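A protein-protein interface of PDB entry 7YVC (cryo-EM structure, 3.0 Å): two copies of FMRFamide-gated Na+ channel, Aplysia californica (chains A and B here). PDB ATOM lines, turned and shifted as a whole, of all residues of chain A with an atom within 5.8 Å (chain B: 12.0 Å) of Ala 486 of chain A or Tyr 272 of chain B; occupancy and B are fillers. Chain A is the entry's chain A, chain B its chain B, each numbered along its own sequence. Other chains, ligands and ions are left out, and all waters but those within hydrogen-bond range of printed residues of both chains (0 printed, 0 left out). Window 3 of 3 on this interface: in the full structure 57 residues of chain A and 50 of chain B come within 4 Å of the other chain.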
ATOM      1  N   PHE A 453      15.406  27.094   0.581  1.00  0.00           N
ATOM      2  CA  PHE A 453      15.257  26.564  -0.768  1.00  0.00           C
ATOM      3  C   PHE A 453      13.907  25.894  -0.970  1.00  0.00           C
ATOM      4  O   PHE A 453      13.399  25.856  -2.093  1.00  0.00           O
ATOM      5  CB  PHE A 453      16.389  25.579  -1.051  1.00  0.00           C
ATOM      6  CG  PHE A 453      16.472  25.142  -2.478  1.00  0.00           C
ATOM      7  CD1 PHE A 453      16.465  26.066  -3.500  1.00  0.00           C
ATOM      8  CD2 PHE A 453      16.570  23.803  -2.795  1.00  0.00           C
ATOM      9  CE1 PHE A 453      16.546  25.662  -4.810  1.00  0.00           C
ATOM     10  CE2 PHE A 453      16.649  23.396  -4.101  1.00  0.00           C
ATOM     11  CZ  PHE A 453      16.639  24.325  -5.110  1.00  0.00           C
ATOM     12  N   LEU A 456       9.133  28.308  -0.530  1.00  0.00           N
ATOM     13  CA  LEU A 456       8.077  28.749  -1.435  1.00  0.00           C
ATOM     14  C   LEU A 456       7.088  27.632  -1.730  1.00  0.00           C
ATOM     15  O   LEU A 456       5.879  27.796  -1.532  1.00  0.00           O
ATOM     16  CB  LEU A 456       8.686  29.272  -2.734  1.00  0.00           C
ATOM     17  CG  LEU A 456       7.714  29.533  -3.884  1.00  0.00           C
ATOM     18  CD1 LEU A 456       6.608  30.482  -3.467  1.00  0.00           C
ATOM     19  CD2 LEU A 456       8.460  30.083  -5.079  1.00  0.00           C
ATOM     20  N   SER A 457       7.585  26.474  -2.162  1.00  0.00           N
ATOM     21  CA  SER A 457       6.675  25.383  -2.486  1.00  0.00           C
ATOM     22  C   SER A 457       5.835  25.005  -1.277  1.00  0.00           C
ATOM     23  O   SER A 457       4.614  24.847  -1.389  1.00  0.00           O
ATOM     24  CB  SER A 457       7.448  24.176  -3.001  1.00  0.00           C
ATOM     25  OG  SER A 457       7.940  23.400  -1.932  1.00  0.00           O
ATOM     26  N   GLU A 460       3.243  27.439  -0.955  1.00  0.00           N
ATOM     27  CA  GLU A 460       2.249  27.244  -2.002  1.00  0.00           C
ATOM     28  C   GLU A 460       1.173  26.266  -1.569  1.00  0.00           C
ATOM     29  O   GLU A 460       0.008  26.424  -1.943  1.00  0.00           O
ATOM     30  CB  GLU A 460       2.915  26.751  -3.283  1.00  0.00           C
ATOM     31  CG  GLU A 460       3.358  27.853  -4.216  1.00  0.00           C
ATOM     32  CD  GLU A 460       3.878  27.322  -5.534  1.00  0.00           C
ATOM     33  OE1 GLU A 460       3.956  26.085  -5.687  1.00  0.00           O
ATOM     34  OE2 GLU A 460       4.211  28.139  -6.416  1.00  0.00           O
ATOM     35  N   PHE A 481       6.838  37.907  -1.773  1.00  0.00           N
ATOM     36  CA  PHE A 481       8.280  38.058  -1.918  1.00  0.00           C
ATOM     37  C   PHE A 481       8.896  36.839  -2.586  1.00  0.00           C
ATOM     38  O   PHE A 481       9.730  36.966  -3.487  1.00  0.00           O
ATOM     39  CB  PHE A 481       8.920  38.296  -0.552  1.00  0.00           C
ATOM     40  CG  PHE A 481       8.703  39.676  -0.016  1.00  0.00           C
ATOM     41  CD1 PHE A 481       8.072  40.638  -0.780  1.00  0.00           C
ATOM     42  CD2 PHE A 481       9.131  40.011   1.252  1.00  0.00           C
ATOM     43  CE1 PHE A 481       7.873  41.907  -0.288  1.00  0.00           C
ATOM     44  CE2 PHE A 481       8.938  41.278   1.747  1.00  0.00           C
ATOM     45  CZ  PHE A 481       8.307  42.229   0.978  1.00  0.00           C
ATOM     46  N   LEU A 482       8.493  35.643  -2.161  1.00  0.00           N
ATOM     47  CA  LEU A 482       9.087  34.440  -2.732  1.00  0.00           C
ATOM     48  C   LEU A 482       8.707  34.276  -4.198  1.00  0.00           C
ATOM     49  O   LEU A 482       9.536  33.859  -5.015  1.00  0.00           O
ATOM     50  CB  LEU A 482       8.678  33.221  -1.915  1.00  0.00           C
ATOM     51  CG  LEU A 482       9.248  33.214  -0.499  1.00  0.00           C
ATOM     52  CD1 LEU A 482       9.054  31.870   0.152  1.00  0.00           C
ATOM     53  CD2 LEU A 482      10.711  33.582  -0.525  1.00  0.00           C
ATOM     54  N   SER A 483       7.461  34.601  -4.555  1.00  0.00           N
ATOM     55  CA  SER A 483       7.047  34.525  -5.951  1.00  0.00           C
ATOM     56  C   SER A 483       7.806  35.533  -6.801  1.00  0.00           C
ATOM     57  O   SER A 483       8.215  35.227  -7.926  1.00  0.00           O
ATOM     58  CB  SER A 483       5.541  34.748  -6.063  1.00  0.00           C
ATOM     59  OG  SER A 483       4.828  33.581  -5.699  1.00  0.00           O
ATOM     60  N   ARG A 484       8.004  36.747  -6.283  1.00  0.00           N
ATOM     61  CA  ARG A 484       8.787  37.728  -7.023  1.00  0.00           C
ATOM     62  C   ARG A 484      10.258  37.350  -7.105  1.00  0.00           C
ATOM     63  O   ARG A 484      10.961  37.838  -7.992  1.00  0.00           O
ATOM     64  CB  ARG A 484       8.640  39.111  -6.395  1.00  0.00           C
ATOM     65  CG  ARG A 484       7.268  39.724  -6.584  1.00  0.00           C
ATOM     66  CD  ARG A 484       7.349  41.236  -6.649  1.00  0.00           C
ATOM     67  NE  ARG A 484       8.435  41.765  -5.832  1.00  0.00           N
ATOM     68  CZ  ARG A 484       8.262  42.586  -4.804  1.00  0.00           C
ATOM     69  NH1 ARG A 484       7.041  42.976  -4.463  1.00  0.00           N
ATOM     70  NH2 ARG A 484       9.308  43.018  -4.115  1.00  0.00           N
ATOM     71  N   LEU A 485      10.749  36.526  -6.185  1.00  0.00           N
ATOM     72  CA  LEU A 485      12.105  36.010  -6.329  1.00  0.00           C
ATOM     73  C   LEU A 485      12.182  34.928  -7.397  1.00  0.00           C
ATOM     74  O   LEU A 485      13.112  34.918  -8.209  1.00  0.00           O
ATOM     75  CB  LEU A 485      12.609  35.455  -5.000  1.00  0.00           C
ATOM     76  CG  LEU A 485      12.825  36.456  -3.871  1.00  0.00           C
ATOM     77  CD1 LEU A 485      13.695  35.851  -2.793  1.00  0.00           C
ATOM     78  CD2 LEU A 485      13.428  37.723  -4.411  1.00  0.00           C
ATOM     79  N   ALA A 486      11.214  34.011  -7.411  1.00  0.00           N
ATOM     80  CA  ALA A 486      11.322  32.838  -8.270  1.00  0.00           C
ATOM     81  C   ALA A 486      11.101  33.188  -9.737  1.00  0.00           C
ATOM     82  O   ALA A 486      11.852  32.737 -10.609  1.00  0.00           O
ATOM     83  CB  ALA A 486      10.330  31.768  -7.821  1.00  0.00           C
ATOM     84  N   HIS A 487      10.073  33.992 -10.034  1.00  0.00           N
ATOM     85  CA  HIS A 487       9.670  34.156 -11.432  1.00  0.00           C
ATOM     86  C   HIS A 487      10.653  35.016 -12.216  1.00  0.00           C
ATOM     87  O   HIS A 487      11.229  34.522 -13.201  1.00  0.00           O
ATOM     88  CB  HIS A 487       8.231  34.673 -11.502  1.00  0.00           C
ATOM     89  CG  HIS A 487       7.206  33.643 -11.146  1.00  0.00           C
ATOM     90  ND1 HIS A 487       5.947  33.619 -11.706  1.00  0.00           N
ATOM     91  CD2 HIS A 487       7.255  32.596 -10.288  1.00  0.00           C
ATOM     92  CE1 HIS A 487       5.264  32.606 -11.206  1.00  0.00           C
ATOM     93  NE2 HIS A 487       6.036  31.969 -10.343  1.00  0.00           N
ATOM     94  N   PRO A 488      10.904  36.289 -11.856  1.00  0.00           N
ATOM     95  CA  PRO A 488      11.938  36.959 -12.648  1.00  0.00           C
ATOM     96  C   PRO A 488      13.343  36.667 -12.134  1.00  0.00           C
ATOM     97  O   PRO A 488      13.685  35.497 -11.967  1.00  0.00           O
ATOM     98  CB  PRO A 488      11.595  38.437 -12.484  1.00  0.00           C
ATOM     99  CG  PRO A 488      10.985  38.518 -11.137  1.00  0.00           C
ATOM    100  CD  PRO A 488      10.257  37.219 -10.911  1.00  0.00           C
ATOM    101  N   LEU B 149      24.030  20.980  -2.312  1.00  0.00           N
ATOM    102  CA  LEU B 149      23.680  21.350  -3.677  1.00  0.00           C
ATOM    103  C   LEU B 149      24.831  22.070  -4.369  1.00  0.00           C
ATOM    104  O   LEU B 149      24.992  21.960  -5.588  1.00  0.00           O
ATOM    105  CB  LEU B 149      22.422  22.217  -3.690  1.00  0.00           C
ATOM    106  CG  LEU B 149      21.057  21.523  -3.643  1.00  0.00           C
ATOM    107  CD1 LEU B 149      20.868  20.633  -4.858  1.00  0.00           C
ATOM    108  CD2 LEU B 149      20.838  20.747  -2.357  1.00  0.00           C
ATOM    109  N   ARG B 153      26.537  21.536  -7.999  1.00  0.00           N
ATOM    110  CA  ARG B 153      26.676  22.606  -8.980  1.00  0.00           C
ATOM    111  C   ARG B 153      28.100  22.694  -9.513  1.00  0.00           C
ATOM    112  O   ARG B 153      28.309  22.848 -10.720  1.00  0.00           O
ATOM    113  CB  ARG B 153      26.241  23.943  -8.383  1.00  0.00           C
ATOM    114  CG  ARG B 153      24.739  24.142  -8.366  1.00  0.00           C
ATOM    115  CD  ARG B 153      24.292  24.784  -7.078  1.00  0.00           C
ATOM    116  NE  ARG B 153      22.855  25.021  -7.059  1.00  0.00           N
ATOM    117  CZ  ARG B 153      22.222  25.642  -6.072  1.00  0.00           C
ATOM    118  NH1 ARG B 153      20.909  25.818  -6.131  1.00  0.00           N
ATOM    119  NH2 ARG B 153      22.902  26.086  -5.025  1.00  0.00           N
ATOM    120  N   ASN B 183      14.242  10.120  -7.056  1.00  0.00           N
ATOM    121  CA  ASN B 183      14.732  11.410  -6.592  1.00  0.00           C
ATOM    122  C   ASN B 183      15.408  11.327  -5.231  1.00  0.00           C
ATOM    123  O   ASN B 183      16.035  12.302  -4.808  1.00  0.00           O
ATOM    124  CB  ASN B 183      13.580  12.412  -6.525  1.00  0.00           C
ATOM    125  CG  ASN B 183      13.139  12.887  -7.892  1.00  0.00           C
ATOM    126  OD1 ASN B 183      13.948  13.013  -8.811  1.00  0.00           O
ATOM    127  ND2 ASN B 183      11.847  13.152  -8.036  1.00  0.00           N
ATOM    128  N   ASP B 265      23.904  26.075   2.216  1.00  0.00           N
ATOM    129  CA  ASP B 265      24.263  26.675   0.939  1.00  0.00           C
ATOM    130  C   ASP B 265      23.197  27.662   0.492  1.00  0.00           C
ATOM    131  O   ASP B 265      22.004  27.454   0.726  1.00  0.00           O
ATOM    132  CB  ASP B 265      24.462  25.606  -0.136  1.00  0.00           C
ATOM    133  CG  ASP B 265      23.199  24.828  -0.422  1.00  0.00           C
ATOM    134  OD1 ASP B 265      22.976  23.793   0.240  1.00  0.00           O
ATOM    135  OD2 ASP B 265      22.427  25.249  -1.308  1.00  0.00           O
ATOM    136  N   GLU B 266      23.639  28.735  -0.152  1.00  0.00           N
ATOM    137  CA  GLU B 266      22.732  29.763  -0.643  1.00  0.00           C
ATOM    138  C   GLU B 266      22.107  29.328  -1.963  1.00  0.00           C
ATOM    139  O   GLU B 266      22.838  29.012  -2.907  1.00  0.00           O
ATOM    140  CB  GLU B 266      23.477  31.076  -0.829  1.00  0.00           C
ATOM    141  CG  GLU B 266      22.610  32.234  -1.304  1.00  0.00           C
ATOM    142  CD  GLU B 266      21.556  32.646  -0.300  1.00  0.00           C
ATOM    143  OE1 GLU B 266      21.761  32.418   0.909  1.00  0.00           O
ATOM    144  OE2 GLU B 266      20.522  33.201  -0.722  1.00  0.00           O
ATOM    145  N   PRO B 267      20.781  29.296  -2.072  1.00  0.00           N
ATOM    146  CA  PRO B 267      20.157  28.930  -3.347  1.00  0.00           C
ATOM    147  C   PRO B 267      20.383  29.993  -4.408  1.00  0.00           C
ATOM    148  O   PRO B 267      20.593  31.169  -4.111  1.00  0.00           O
ATOM    149  CB  PRO B 267      18.671  28.808  -2.992  1.00  0.00           C
ATOM    150  CG  PRO B 267      18.502  29.657  -1.785  1.00  0.00           C
ATOM    151  CD  PRO B 267      19.785  29.554  -1.020  1.00  0.00           C
ATOM    152  N   LEU B 268      20.339  29.556  -5.664  1.00  0.00           N
ATOM    153  CA  LEU B 268      20.510  30.460  -6.784  1.00  0.00           C
ATOM    154  C   LEU B 268      19.290  31.369  -6.923  1.00  0.00           C
ATOM    155  O   LEU B 268      18.196  31.025  -6.475  1.00  0.00           O
ATOM    156  CB  LEU B 268      20.740  29.668  -8.066  1.00  0.00           C
ATOM    157  CG  LEU B 268      22.054  28.891  -8.106  1.00  0.00           C
ATOM    158  CD1 LEU B 268      22.290  28.307  -9.489  1.00  0.00           C
ATOM    159  CD2 LEU B 268      23.212  29.773  -7.683  1.00  0.00           C
ATOM    160  N   PRO B 269      19.459  32.546  -7.535  1.00  0.00           N
ATOM    161  CA  PRO B 269      18.364  33.530  -7.546  1.00  0.00           C
ATOM    162  C   PRO B 269      17.076  33.041  -8.188  1.00  0.00           C
ATOM    163  O   PRO B 269      15.993  33.448  -7.752  1.00  0.00           O
ATOM    164  CB  PRO B 269      18.962  34.708  -8.328  1.00  0.00           C
ATOM    165  CG  PRO B 269      20.132  34.143  -9.059  1.00  0.00           C
ATOM    166  CD  PRO B 269      20.675  33.083  -8.165  1.00  0.00           C
ATOM    167  N   GLY B 270      17.150  32.195  -9.209  1.00  0.00           N
ATOM    168  CA  GLY B 270      15.952  31.833  -9.939  1.00  0.00           C
ATOM    169  C   GLY B 270      15.400  30.450  -9.664  1.00  0.00           C
ATOM    170  O   GLY B 270      14.337  30.097 -10.180  1.00  0.00           O
ATOM    171  N   THR B 271      16.098  29.657  -8.861  1.00  0.00           N
ATOM    172  CA  THR B 271      15.699  28.284  -8.603  1.00  0.00           C
ATOM    173  C   THR B 271      15.047  28.156  -7.234  1.00  0.00           C
ATOM    174  O   THR B 271      15.409  28.854  -6.284  1.00  0.00           O
ATOM    175  CB  THR B 271      16.897  27.336  -8.688  1.00  0.00           C
ATOM    176  OG1 THR B 271      17.960  27.832  -7.868  1.00  0.00           O
ATOM    177  CG2 THR B 271      17.381  27.216 -10.117  1.00  0.00           C
ATOM    178  N   TYR B 272      14.075  27.254  -7.145  1.00  0.00           N
ATOM    179  CA  TYR B 272      13.416  26.942  -5.888  1.00  0.00           C
ATOM    180  C   TYR B 272      13.209  25.437  -5.801  1.00  0.00           C
ATOM    181  O   TYR B 272      13.178  24.735  -6.812  1.00  0.00           O
ATOM    182  CB  TYR B 272      12.092  27.710  -5.740  1.00  0.00           C
ATOM    183  CG  TYR B 272      10.983  27.329  -6.702  1.00  0.00           C
ATOM    184  CD1 TYR B 272      10.285  26.137  -6.567  1.00  0.00           C
ATOM    185  CD2 TYR B 272      10.621  28.179  -7.735  1.00  0.00           C
ATOM    186  CE1 TYR B 272       9.273  25.798  -7.438  1.00  0.00           C
ATOM    187  CE2 TYR B 272       9.609  27.849  -8.610  1.00  0.00           C
ATOM    188  CZ  TYR B 272       8.939  26.659  -8.456  1.00  0.00           C
ATOM    189  OH  TYR B 272       7.929  26.328  -9.327  1.00  0.00           O
ATOM    190  N   GLY B 273      13.078  24.948  -4.574  1.00  0.00           N
ATOM    191  CA  GLY B 273      12.917  23.529  -4.349  1.00  0.00           C
ATOM    192  C   GLY B 273      11.470  23.116  -4.227  1.00  0.00           C
ATOM    193  O   GLY B 273      10.563  23.941  -4.193  1.00  0.00           O
ATOM    194  N   VAL B 274      11.260  21.806  -4.153  1.00  0.00           N
ATOM    195  CA  VAL B 274       9.928  21.224  -4.060  1.00  0.00           C
ATOM    196  C   VAL B 274       9.817  20.515  -2.721  1.00  0.00           C
ATOM    197  O   VAL B 274      10.562  19.564  -2.454  1.00  0.00           O
ATOM    198  CB  VAL B 274       9.644  20.258  -5.218  1.00  0.00           C
ATOM    199  CG1 VAL B 274       8.336  19.535  -4.992  1.00  0.00           C
ATOM    200  CG2 VAL B 274       9.611  21.011  -6.529  1.00  0.00           C
ATOM    201  N   TYR B 275       8.886  20.965  -1.888  1.00  0.00           N
ATOM    202  CA  TYR B 275       8.682  20.350  -0.584  1.00  0.00           C
ATOM    203  C   TYR B 275       8.060  18.977  -0.776  1.00  0.00           C
ATOM    204  O   TYR B 275       6.919  18.861  -1.230  1.00  0.00           O
ATOM    205  CB  TYR B 275       7.800  21.233   0.291  1.00  0.00           C
ATOM    206  CG  TYR B 275       7.898  20.924   1.764  1.00  0.00           C
ATOM    207  CD1 TYR B 275       7.270  19.816   2.299  1.00  0.00           C
ATOM    208  CD2 TYR B 275       8.621  21.735   2.615  1.00  0.00           C
ATOM    209  CE1 TYR B 275       7.356  19.526   3.636  1.00  0.00           C
ATOM    210  CE2 TYR B 275       8.712  21.450   3.954  1.00  0.00           C
ATOM    211  CZ  TYR B 275       8.077  20.344   4.456  1.00  0.00           C
ATOM    212  OH  TYR B 275       8.162  20.049   5.791  1.00  0.00           O
ATOM    213  N   ASN B 276       8.811  17.936  -0.441  1.00  0.00           N
ATOM    214  CA  ASN B 276       8.305  16.571  -0.497  1.00  0.00           C
ATOM    215  C   ASN B 276       7.348  16.365   0.665  1.00  0.00           C
ATOM    216  O   ASN B 276       7.763  16.029   1.775  1.00  0.00           O
ATOM    217  CB  ASN B 276       9.461  15.579  -0.445  1.00  0.00           C
ATOM    218  CG  ASN B 276       9.025  14.159  -0.718  1.00  0.00           C
ATOM    219  OD1 ASN B 276       7.840  13.876  -0.859  1.00  0.00           O
ATOM    220  ND2 ASN B 276       9.988  13.252  -0.795  1.00  0.00           N
ATOM    221  N   PHE B 277       6.062  16.556   0.419  1.00  0.00           N
ATOM    222  CA  PHE B 277       5.088  16.425   1.497  1.00  0.00           C
ATOM    223  C   PHE B 277       4.834  15.011   1.881  1.00  0.00           C
ATOM    224  O   PHE B 277       3.942  14.765   2.688  1.00  0.00           O
ATOM    225  CB  PHE B 277       3.780  17.103   1.099  1.00  0.00           C
ATOM    226  CG  PHE B 277       3.710  18.542   1.497  1.00  0.00           C
ATOM    227  CD1 PHE B 277       3.501  18.896   2.811  1.00  0.00           C
ATOM    228  CD2 PHE B 277       3.871  19.538   0.560  1.00  0.00           C
ATOM    229  CE1 PHE B 277       3.445  20.215   3.179  1.00  0.00           C
ATOM    230  CE2 PHE B 277       3.818  20.856   0.925  1.00  0.00           C
ATOM    231  CZ  PHE B 277       3.602  21.195   2.235  1.00  0.00           C
ATOM    232  N   HIS B 283      14.078  18.575   4.668  1.00  0.00           N
ATOM    233  CA  HIS B 283      13.977  20.030   4.616  1.00  0.00           C
ATOM    234  C   HIS B 283      14.218  20.684   5.970  1.00  0.00           C
ATOM    235  O   HIS B 283      13.632  21.721   6.274  1.00  0.00           O
ATOM    236  CB  HIS B 283      12.633  20.468   4.036  1.00  0.00           C
ATOM    237  CG  HIS B 283      12.214  19.671   2.844  1.00  0.00           C
ATOM    238  ND1 HIS B 283      13.020  19.508   1.740  1.00  0.00           N
ATOM    239  CD2 HIS B 283      11.085  18.969   2.591  1.00  0.00           C
ATOM    240  CE1 HIS B 283      12.402  18.749   0.854  1.00  0.00           C
ATOM    241  NE2 HIS B 283      11.226  18.409   1.346  1.00  0.00           N
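Of chain B, only Gly 270 (3.7 Å) and Tyr 272 (3.6 Å) come within 4 Å of Ala 486 of chain A. Of chain B, only Pro 267 (3.6 Å), Thr 271 (3.7 Å), Tyr 272 (3.5 Å) and Gly 273 (2.7 Å) come within 4 Å of Phe 453 of chain A. Of the printed residues of chain B, Leu 456 of chain A touches Tyr 272. No residue of chain B comes within 4 Å of Pro 488 of chain A. Of the printed residues of chain A, Pro 269 of chain B touches Leu 485. Printed residues of chain A within 4 Å of Thr 271 of chain B: Phe 453 (3.7 Å). Of the printed residues of chain A, Tyr 275 of chain B touches Ser 457 (2.6 Å). The nearest residue of chain B that does not touch Ala 486 of chain A is Pro 269 of chain B (4.7 Å). The nearest residue of chain A that does not touch Tyr 272 of chain B is Ser 457 of chain A (5.0 Å).
No position is printed for both chains. Of the 11 pairs that touch across the chains among the printed residues, none has its exchanged pair printed and touching as well.
OG of Ser 457 of chain A sits at hydrogen-bond distance from N of Tyr 275 of chain B, at 2.6 Å. The backbone carbonyl oxygen (O) of Pro 269 of chain B lies close to the backbone carbonyl oxygen (O) of Leu 485 of chain A (3.3 Å). The backbone carbonyl oxygen (O) of Phe 453 of chain A is in hydrogen-bond range of the backbone NH (N) of Gly 273 of chain B (2.7 Å).
The side-chain hydroxyl of Thr 271 of chain B sits close to the backbone carbonyl oxygen of Leu 268 of chain B (3.5 Å).
Among the printed residues, merely in contact across the chains: Phe 453 of chain A with Pro 267 of chain B (3.6 Å), Phe 453 of chain A with Thr 271 of chain B (3.7 Å), Phe 453 of chain A with Tyr 272 of chain B (3.5 Å), Leu 456 of chain A with Tyr 272 of chain B (3.9 Å), Ser 457 of chain A with Gly 273 of chain B (3.3 Å), Ser 457 of chain A with Val 274 of chain B (3.5 Å), Ala 486 of chain A with Gly 270 of chain B (3.7 Å) and Ala 486 of chain A with Tyr 272 of chain B (3.6 Å).
Hydrophobic or aromatic side chains of chain B within 4 Å of the printed part of chain A: Pro 267, Tyr 272 and Tyr 275. Of the 12 printed residues of chain A, 5 touch a printed residue of chain B. Printed residues of chain A that touch a printed residue of chain B: Phe 453, Leu 456, Ser 457, Leu 485 and Ala 486. Among the printed residues, 11 pairs touch across the chains. Among the printed residues, no Asp or Glu carboxylate lies within 4 Å of a Lys or Arg side-chain nitrogen of the other chain.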
